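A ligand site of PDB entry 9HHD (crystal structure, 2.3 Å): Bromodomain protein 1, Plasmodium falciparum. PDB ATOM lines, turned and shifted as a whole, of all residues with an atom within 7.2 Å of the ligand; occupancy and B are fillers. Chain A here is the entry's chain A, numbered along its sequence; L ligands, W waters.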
ATOM      1  N   HIS A  31       5.318   6.578  10.496  1.00  0.00           N
ATOM      2  CA  HIS A  31       3.903   6.238  10.630  1.00  0.00           C
ATOM      3  C   HIS A  31       3.451   5.163   9.642  1.00  0.00           C
ATOM      4  O   HIS A  31       2.375   4.593   9.832  1.00  0.00           O
ATOM      5  CB  HIS A  31       3.065   7.481  10.419  1.00  0.00           C
ATOM      6  CG  HIS A  31       3.139   7.974   9.026  1.00  0.00           C
ATOM      7  ND1 HIS A  31       4.137   8.816   8.587  1.00  0.00           N
ATOM      8  CD2 HIS A  31       2.390   7.680   7.932  1.00  0.00           C
ATOM      9  CE1 HIS A  31       3.985   9.053   7.301  1.00  0.00           C
ATOM     10  NE2 HIS A  31       2.927   8.369   6.879  1.00  0.00           N
ATOM     11  N   ILE A  32       4.208   4.903   8.574  1.00  0.00           N
ATOM     12  CA  ILE A  32       3.789   3.849   7.648  1.00  0.00           C
ATOM     13  C   ILE A  32       4.150   2.469   8.166  1.00  0.00           C
ATOM     14  O   ILE A  32       3.614   1.467   7.666  1.00  0.00           O
ATOM     15  CB  ILE A  32       4.389   4.055   6.242  1.00  0.00           C
ATOM     16  CG1 ILE A  32       5.842   3.612   6.163  1.00  0.00           C
ATOM     17  CG2 ILE A  32       4.284   5.516   5.815  1.00  0.00           C
ATOM     18  CD1 ILE A  32       6.491   3.942   4.851  1.00  0.00           C
ATOM     19  N   PHE A  33       5.028   2.384   9.161  1.00  0.00           N
ATOM     20  CA  PHE A  33       5.365   1.120   9.809  1.00  0.00           C
ATOM     21  C   PHE A  33       4.635   0.926  11.130  1.00  0.00           C
ATOM     22  O   PHE A  33       4.826  -0.109  11.773  1.00  0.00           O
ATOM     23  CB  PHE A  33       6.873   1.052  10.030  1.00  0.00           C
ATOM     24  CG  PHE A  33       7.652   1.190   8.758  1.00  0.00           C
ATOM     25  CD1 PHE A  33       7.687   0.163   7.842  1.00  0.00           C
ATOM     26  CD2 PHE A  33       8.335   2.345   8.478  1.00  0.00           C
ATOM     27  CE1 PHE A  33       8.399   0.268   6.673  1.00  0.00           C
ATOM     28  CE2 PHE A  33       9.043   2.476   7.283  1.00  0.00           C
ATOM     29  CZ  PHE A  33       9.076   1.435   6.392  1.00  0.00           C
ATOM     30  N   GLU A  34       3.793   1.879  11.544  1.00  0.00           N
ATOM     31  CA  GLU A  34       3.194   1.821  12.868  1.00  0.00           C
ATOM     32  C   GLU A  34       2.255   0.633  13.001  1.00  0.00           C
ATOM     33  O   GLU A  34       2.317  -0.113  13.978  1.00  0.00           O
ATOM     34  CB  GLU A  34       2.459   3.121  13.171  1.00  0.00           C
ATOM     35  CG  GLU A  34       1.854   3.154  14.567  1.00  0.00           C
ATOM     36  CD  GLU A  34       2.897   3.122  15.677  1.00  0.00           C
ATOM     37  OE1 GLU A  34       4.072   3.472  15.413  1.00  0.00           O
ATOM     38  OE2 GLU A  34       2.555   2.742  16.824  1.00  0.00           O
ATOM     39  N   LYS A  35       1.372   0.448  12.017  1.00  0.00           N
ATOM     40  CA  LYS A  35       0.369  -0.596  12.059  1.00  0.00           C
ATOM     41  C   LYS A  35       0.589  -1.587  10.923  1.00  0.00           C
ATOM     42  O   LYS A  35       1.275  -1.291   9.949  1.00  0.00           O
ATOM     43  CB  LYS A  35      -1.038  -0.009  11.985  1.00  0.00           C
ATOM     44  CG  LYS A  35      -1.274   1.084  13.013  1.00  0.00           C
ATOM     45  CD  LYS A  35      -2.730   1.506  13.024  1.00  0.00           C
ATOM     46  CE  LYS A  35      -2.956   2.681  13.976  1.00  0.00           C
ATOM     47  NZ  LYS A  35      -2.388   2.372  15.336  1.00  0.00           N
ATOM     48  N   LEU A  36      -0.010  -2.771  11.059  1.00  0.00           N
ATOM     49  CA  LEU A  36       0.034  -3.734   9.977  1.00  0.00           C
ATOM     50  C   LEU A  36      -0.692  -3.175   8.766  1.00  0.00           C
ATOM     51  O   LEU A  36      -1.688  -2.454   8.890  1.00  0.00           O
ATOM     52  CB  LEU A  36      -0.587  -5.057  10.406  1.00  0.00           C
ATOM     53  CG  LEU A  36       0.231  -5.833  11.439  1.00  0.00           C
ATOM     54  CD1 LEU A  36      -0.513  -7.082  11.880  1.00  0.00           C
ATOM     55  CD2 LEU A  36       1.601  -6.186  10.879  1.00  0.00           C
ATOM     56  N   VAL A  37      -0.177  -3.497   7.578  1.00  0.00           N
ATOM     57  CA  VAL A  37      -0.783  -2.989   6.360  1.00  0.00           C
ATOM     58  C   VAL A  37      -2.172  -3.587   6.191  1.00  0.00           C
ATOM     59  O   VAL A  37      -2.364  -4.798   6.360  1.00  0.00           O
ATOM     60  CB  VAL A  37       0.106  -3.293   5.145  1.00  0.00           C
ATOM     61  CG1 VAL A  37      -0.530  -2.796   3.862  1.00  0.00           C
ATOM     62  CG2 VAL A  37       1.498  -2.689   5.332  1.00  0.00           C
ATOM     63  N   ASP A  38      -3.158  -2.743   5.925  1.00  0.00           N
ATOM     64  CA  ASP A  38      -4.471  -3.203   5.475  1.00  0.00           C
ATOM     65  C   ASP A  38      -4.440  -3.216   3.963  1.00  0.00           C
ATOM     66  O   ASP A  38      -4.485  -2.157   3.330  1.00  0.00           O
ATOM     67  CB  ASP A  38      -5.584  -2.295   6.000  1.00  0.00           C
ATOM     68  CG  ASP A  38      -6.955  -2.735   5.524  1.00  0.00           C
ATOM     69  OD1 ASP A  38      -7.364  -3.873   5.847  1.00  0.00           O
ATOM     70  OD2 ASP A  38      -7.636  -1.947   4.831  1.00  0.00           O
ATOM     71  N   LYS A  41      -7.126  -0.855   2.175  1.00  0.00           N
ATOM     72  CA  LYS A  41      -7.008   0.586   2.345  1.00  0.00           C
ATOM     73  C   LYS A  41      -5.717   1.143   1.744  1.00  0.00           C
ATOM     74  O   LYS A  41      -5.680   2.341   1.417  1.00  0.00           O
ATOM     75  CB  LYS A  41      -7.083   0.946   3.836  1.00  0.00           C
ATOM     76  N   GLN A  42      -4.664   0.339   1.621  1.00  0.00           N
ATOM     77  CA  GLN A  42      -3.449   0.724   0.922  1.00  0.00           C
ATOM     78  C   GLN A  42      -3.460   0.286  -0.522  1.00  0.00           C
ATOM     79  O   GLN A  42      -2.466   0.485  -1.229  1.00  0.00           O
ATOM     80  CB  GLN A  42      -2.207   0.157   1.616  1.00  0.00           C
ATOM     81  CG  GLN A  42      -2.060   0.525   3.077  1.00  0.00           C
ATOM     82  CD  GLN A  42      -2.287   1.992   3.332  1.00  0.00           C
ATOM     83  OE1 GLN A  42      -1.935   2.858   2.515  1.00  0.00           O
ATOM     84  NE2 GLN A  42      -2.886   2.293   4.477  1.00  0.00           N
ATOM     85  N   ASN A  43      -4.556  -0.318  -0.970  1.00  0.00           N
ATOM     86  CA  ASN A  43      -4.737  -0.878  -2.311  1.00  0.00           C
ATOM     87  C   ASN A  43      -3.474  -1.563  -2.816  1.00  0.00           C
ATOM     88  O   ASN A  43      -3.048  -1.372  -3.958  1.00  0.00           O
ATOM     89  CB  ASN A  43      -5.226   0.173  -3.296  1.00  0.00           C
ATOM     90  CG  ASN A  43      -6.197  -0.396  -4.299  1.00  0.00           C
ATOM     91  OD1 ASN A  43      -7.155  -1.073  -3.922  1.00  0.00           O
ATOM     92  ND2 ASN A  43      -5.931  -0.177  -5.578  1.00  0.00           N
ATOM     93  N   CYS A  44      -2.882  -2.375  -1.944  1.00  0.00           N
ATOM     94  CA  CYS A  44      -1.867  -3.357  -2.317  1.00  0.00           C
ATOM     95  C   CYS A  44      -2.447  -4.729  -1.966  1.00  0.00           C
ATOM     96  O   CYS A  44      -2.033  -5.367  -0.995  1.00  0.00           O
ATOM     97  CB  CYS A  44      -0.538  -3.103  -1.606  1.00  0.00           C
ATOM     98  SG  CYS A  44      -0.669  -2.852   0.175  1.00  0.00           S
ATOM     99  N   TYR A  47      -0.418  -7.977  -0.677  1.00  0.00           N
ATOM    100  CA  TYR A  47       0.648  -7.777   0.293  1.00  0.00           C
ATOM    101  C   TYR A  47       0.939  -9.031   1.104  1.00  0.00           C
ATOM    102  O   TYR A  47       2.091  -9.421   1.273  1.00  0.00           O
ATOM    103  CB  TYR A  47       0.322  -6.611   1.223  1.00  0.00           C
ATOM    104  CG  TYR A  47       1.453  -6.309   2.165  1.00  0.00           C
ATOM    105  CD1 TYR A  47       2.514  -5.509   1.758  1.00  0.00           C
ATOM    106  CD2 TYR A  47       1.475  -6.835   3.446  1.00  0.00           C
ATOM    107  CE1 TYR A  47       3.556  -5.228   2.617  1.00  0.00           C
ATOM    108  CE2 TYR A  47       2.526  -6.564   4.316  1.00  0.00           C
ATOM    109  CZ  TYR A  47       3.558  -5.751   3.890  1.00  0.00           C
ATOM    110  OH  TYR A  47       4.607  -5.478   4.728  1.00  0.00           O
ATOM    111  N   ILE A  51       4.290 -11.036   1.811  1.00  0.00           N
ATOM    112  CA  ILE A  51       4.797 -10.930   3.176  1.00  0.00           C
ATOM    113  C   ILE A  51       4.064 -11.935   4.043  1.00  0.00           C
ATOM    114  O   ILE A  51       2.892 -11.758   4.385  1.00  0.00           O
ATOM    115  CB  ILE A  51       4.633  -9.502   3.713  1.00  0.00           C
ATOM    116  CG1 ILE A  51       5.382  -8.534   2.812  1.00  0.00           C
ATOM    117  CG2 ILE A  51       5.136  -9.420   5.137  1.00  0.00           C
ATOM    118  CD1 ILE A  51       6.785  -9.000   2.476  1.00  0.00           C
ATOM    119  N   MET A  55       5.044  -7.583  10.327  1.00  0.00           N
ATOM    120  CA  MET A  55       5.512  -6.960  11.560  1.00  0.00           C
ATOM    121  C   MET A  55       5.305  -5.449  11.495  1.00  0.00           C
ATOM    122  O   MET A  55       5.474  -4.846  10.433  1.00  0.00           O
ATOM    123  CB  MET A  55       6.977  -7.321  11.815  1.00  0.00           C
ATOM    124  CG  MET A  55       7.529  -6.886  13.157  1.00  0.00           C
ATOM    125  SD  MET A  55       6.613  -7.556  14.553  1.00  0.00           S
ATOM    126  CE  MET A  55       6.942  -9.313  14.411  1.00  0.00           C
ATOM    127  N   ILE A  82      10.657  -5.700   9.910  1.00  0.00           N
ATOM    128  CA  ILE A  82       9.878  -4.650   9.259  1.00  0.00           C
ATOM    129  C   ILE A  82      10.642  -4.100   8.057  1.00  0.00           C
ATOM    130  O   ILE A  82      10.074  -3.922   6.973  1.00  0.00           O
ATOM    131  CB  ILE A  82       9.565  -3.527  10.271  1.00  0.00           C
ATOM    132  CG1 ILE A  82       8.743  -4.082  11.431  1.00  0.00           C
ATOM    133  CG2 ILE A  82       8.812  -2.421   9.579  1.00  0.00           C
ATOM    134  CD1 ILE A  82       8.465  -3.060  12.506  1.00  0.00           C
ATOM    135  N   ASN A  85      10.806  -6.704   5.222  1.00  0.00           N
ATOM    136  CA  ASN A  85       9.542  -6.796   4.498  1.00  0.00           C
ATOM    137  C   ASN A  85       9.384  -5.595   3.584  1.00  0.00           C
ATOM    138  O   ASN A  85       8.888  -5.727   2.455  1.00  0.00           O
ATOM    139  CB  ASN A  85       8.359  -6.864   5.464  1.00  0.00           C
ATOM    140  CG  ASN A  85       8.252  -8.208   6.188  1.00  0.00           C
ATOM    141  OD1 ASN A  85       8.856  -9.218   5.810  1.00  0.00           O
ATOM    142  ND2 ASN A  85       7.432  -8.224   7.225  1.00  0.00           N
ATOM    143  N   CYS A  86       9.784  -4.427   4.063  1.00  0.00           N
ATOM    144  CA  CYS A  86       9.615  -3.199   3.291  1.00  0.00           C
ATOM    145  C   CYS A  86      10.439  -3.239   2.016  1.00  0.00           C
ATOM    146  O   CYS A  86       9.934  -2.965   0.917  1.00  0.00           O
ATOM    147  CB  CYS A  86      10.005  -1.993   4.149  1.00  0.00           C
ATOM    148  SG  CYS A  86       9.903  -0.365   3.322  1.00  0.00           S
ATOM    149  N   SER A  87      11.729  -3.588   2.140  1.00  0.00           N
ATOM    150  CA  SER A  87      12.563  -3.650   0.944  1.00  0.00           C
ATOM    151  C   SER A  87      12.161  -4.814   0.034  1.00  0.00           C
ATOM    152  O   SER A  87      12.249  -4.697  -1.188  1.00  0.00           O
ATOM    153  CB  SER A  87      14.037  -3.733   1.322  1.00  0.00           C
ATOM    154  OG  SER A  87      14.327  -4.949   1.976  1.00  0.00           O
ATOM    155  N   TYR A  89       8.996  -5.993  -0.451  1.00  0.00           N
ATOM    156  CA  TYR A  89       7.771  -5.715  -1.176  1.00  0.00           C
ATOM    157  C   TYR A  89       7.904  -4.498  -2.102  1.00  0.00           C
ATOM    158  O   TYR A  89       7.403  -4.518  -3.228  1.00  0.00           O
ATOM    159  CB  TYR A  89       6.616  -5.515  -0.203  1.00  0.00           C
ATOM    160  CG  TYR A  89       5.301  -5.354  -0.902  1.00  0.00           C
ATOM    161  CD1 TYR A  89       4.594  -6.466  -1.364  1.00  0.00           C
ATOM    162  CD2 TYR A  89       4.763  -4.098  -1.125  1.00  0.00           C
ATOM    163  CE1 TYR A  89       3.382  -6.324  -2.023  1.00  0.00           C
ATOM    164  CE2 TYR A  89       3.567  -3.945  -1.769  1.00  0.00           C
ATOM    165  CZ  TYR A  89       2.872  -5.055  -2.213  1.00  0.00           C
ATOM    166  OH  TYR A  89       1.672  -4.880  -2.862  1.00  0.00           O
ATOM    167  N   ASN A  90       8.542  -3.433  -1.647  1.00  0.00           N
ATOM    168  CA  ASN A  90       8.573  -2.183  -2.396  1.00  0.00           C
ATOM    169  C   ASN A  90       9.849  -2.089  -3.227  1.00  0.00           C
ATOM    170  O   ASN A  90      10.940  -2.419  -2.759  1.00  0.00           O
ATOM    171  CB  ASN A  90       8.438  -0.985  -1.456  1.00  0.00           C
ATOM    172  CG  ASN A  90       7.288  -1.148  -0.480  1.00  0.00           C
ATOM    173  OD1 ASN A  90       6.171  -0.720  -0.771  1.00  0.00           O
ATOM    174  ND2 ASN A  90       7.551  -1.753   0.686  1.00  0.00           N
ATOM    175  N   VAL A  96       8.233   4.399  -0.470  1.00  0.00           N
ATOM    176  CA  VAL A  96       8.217   3.561   0.723  1.00  0.00           C
ATOM    177  C   VAL A  96       9.564   2.886   0.945  1.00  0.00           C
ATOM    178  O   VAL A  96      10.086   2.876   2.065  1.00  0.00           O
ATOM    179  CB  VAL A  96       7.072   2.534   0.648  1.00  0.00           C
ATOM    180  CG1 VAL A  96       7.232   1.485   1.731  1.00  0.00           C
ATOM    181  CG2 VAL A  96       5.717   3.229   0.757  1.00  0.00           C
ATOM    182  N   ALA A  97      10.142   2.313  -0.113  1.00  0.00           N
ATOM    183  CA  ALA A  97      11.451   1.696   0.049  1.00  0.00           C
ATOM    184  C   ALA A  97      12.476   2.699   0.580  1.00  0.00           C
ATOM    185  O   ALA A  97      13.241   2.388   1.508  1.00  0.00           O
ATOM    186  CB  ALA A  97      11.908   1.077  -1.270  1.00  0.00           C
HETATM  187  C1  LIG L   1       2.190   3.943   2.577  1.00  0.00           C
HETATM  188  C2  LIG L   1       1.344   3.637   3.843  1.00  0.00           C
HETATM  189  C3  LIG L   1       0.430   4.601   4.360  1.00  0.00           C
HETATM  190  C4  LIG L   1      -0.338   4.301   5.517  1.00  0.00           C
HETATM  191  C5  LIG L   1      -0.235   3.061   6.188  1.00  0.00           C
HETATM  192  C6  LIG L   1       0.651   2.102   5.695  1.00  0.00           C
HETATM  193  C7  LIG L   1       1.419   2.369   4.537  1.00  0.00           C
HETATM  194  C8  LIG L   1       2.328   1.304   4.110  1.00  0.00           C
HETATM  195  C9  LIG L   1       4.055  -0.081   4.395  1.00  0.00           C
HETATM  196  C10 LIG L   1       5.194  -0.711   5.134  1.00  0.00           C
HETATM  197  C11 LIG L   1       2.433   0.561   2.885  1.00  0.00           C
HETATM  198  C12 LIG L   1       3.539  -0.322   3.079  1.00  0.00           C
HETATM  199  C13 LIG L   1       1.616   0.578   1.604  1.00  0.00           C
HETATM  200  C14 LIG L   1       2.447   0.764   0.257  1.00  0.00           C
HETATM  201  C15 LIG L   1       3.065  -0.600  -0.291  1.00  0.00           C
HETATM  202  C16 LIG L   1       3.204  -1.686   0.826  1.00  0.00           C
HETATM  203  C17 LIG L   1       4.001  -1.278   2.049  1.00  0.00           C
HETATM  204  N1  LIG L   1       3.310   0.897   4.985  1.00  0.00           N
HETATM  205  O1  LIG L   1       5.123  -1.754   2.194  1.00  0.00           O
HETATM  206  O   HOH W   1      -2.020   6.794   3.301  1.00  0.00           O
HETATM  207  O   HOH W   2      -2.340   0.320   6.328  1.00  0.00           O
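O of Ile 32 sits at hydrogen-bond distance from N1 of the ligand (2.8 Å). ND2 of Asn 90 is in hydrogen-bond range of O1 of the ligand, 2.9 Å away.
ND2 of Asn 90 lies within hydrogen-bond range of O of Cys 86, at 2.7 Å. The backbone carbonyl oxygen of Val 96 lies within hydrogen-bond range of the side-chain sulfur of Cys 86 (3.5 Å).
Merely in contact with the ligand: Gln 42, Tyr 89, Phe 33, Val 37, Tyr 47 and Val 96. Hydrophobic or aromatic side chains that line the ligand: Ile 32, Phe 33, Val 37, Tyr 47, Tyr 89 and Val 96. Of the 23 residues printed, 8 come within 4 Å of the ligand. The nearest printed residue that does not touch the ligand is Cys 44 (4.1 Å).
Water W2 lies within hydrogen-bond range of the side-chain amide nitrogen of Gln 42 and the backbone NH of Asp 38.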
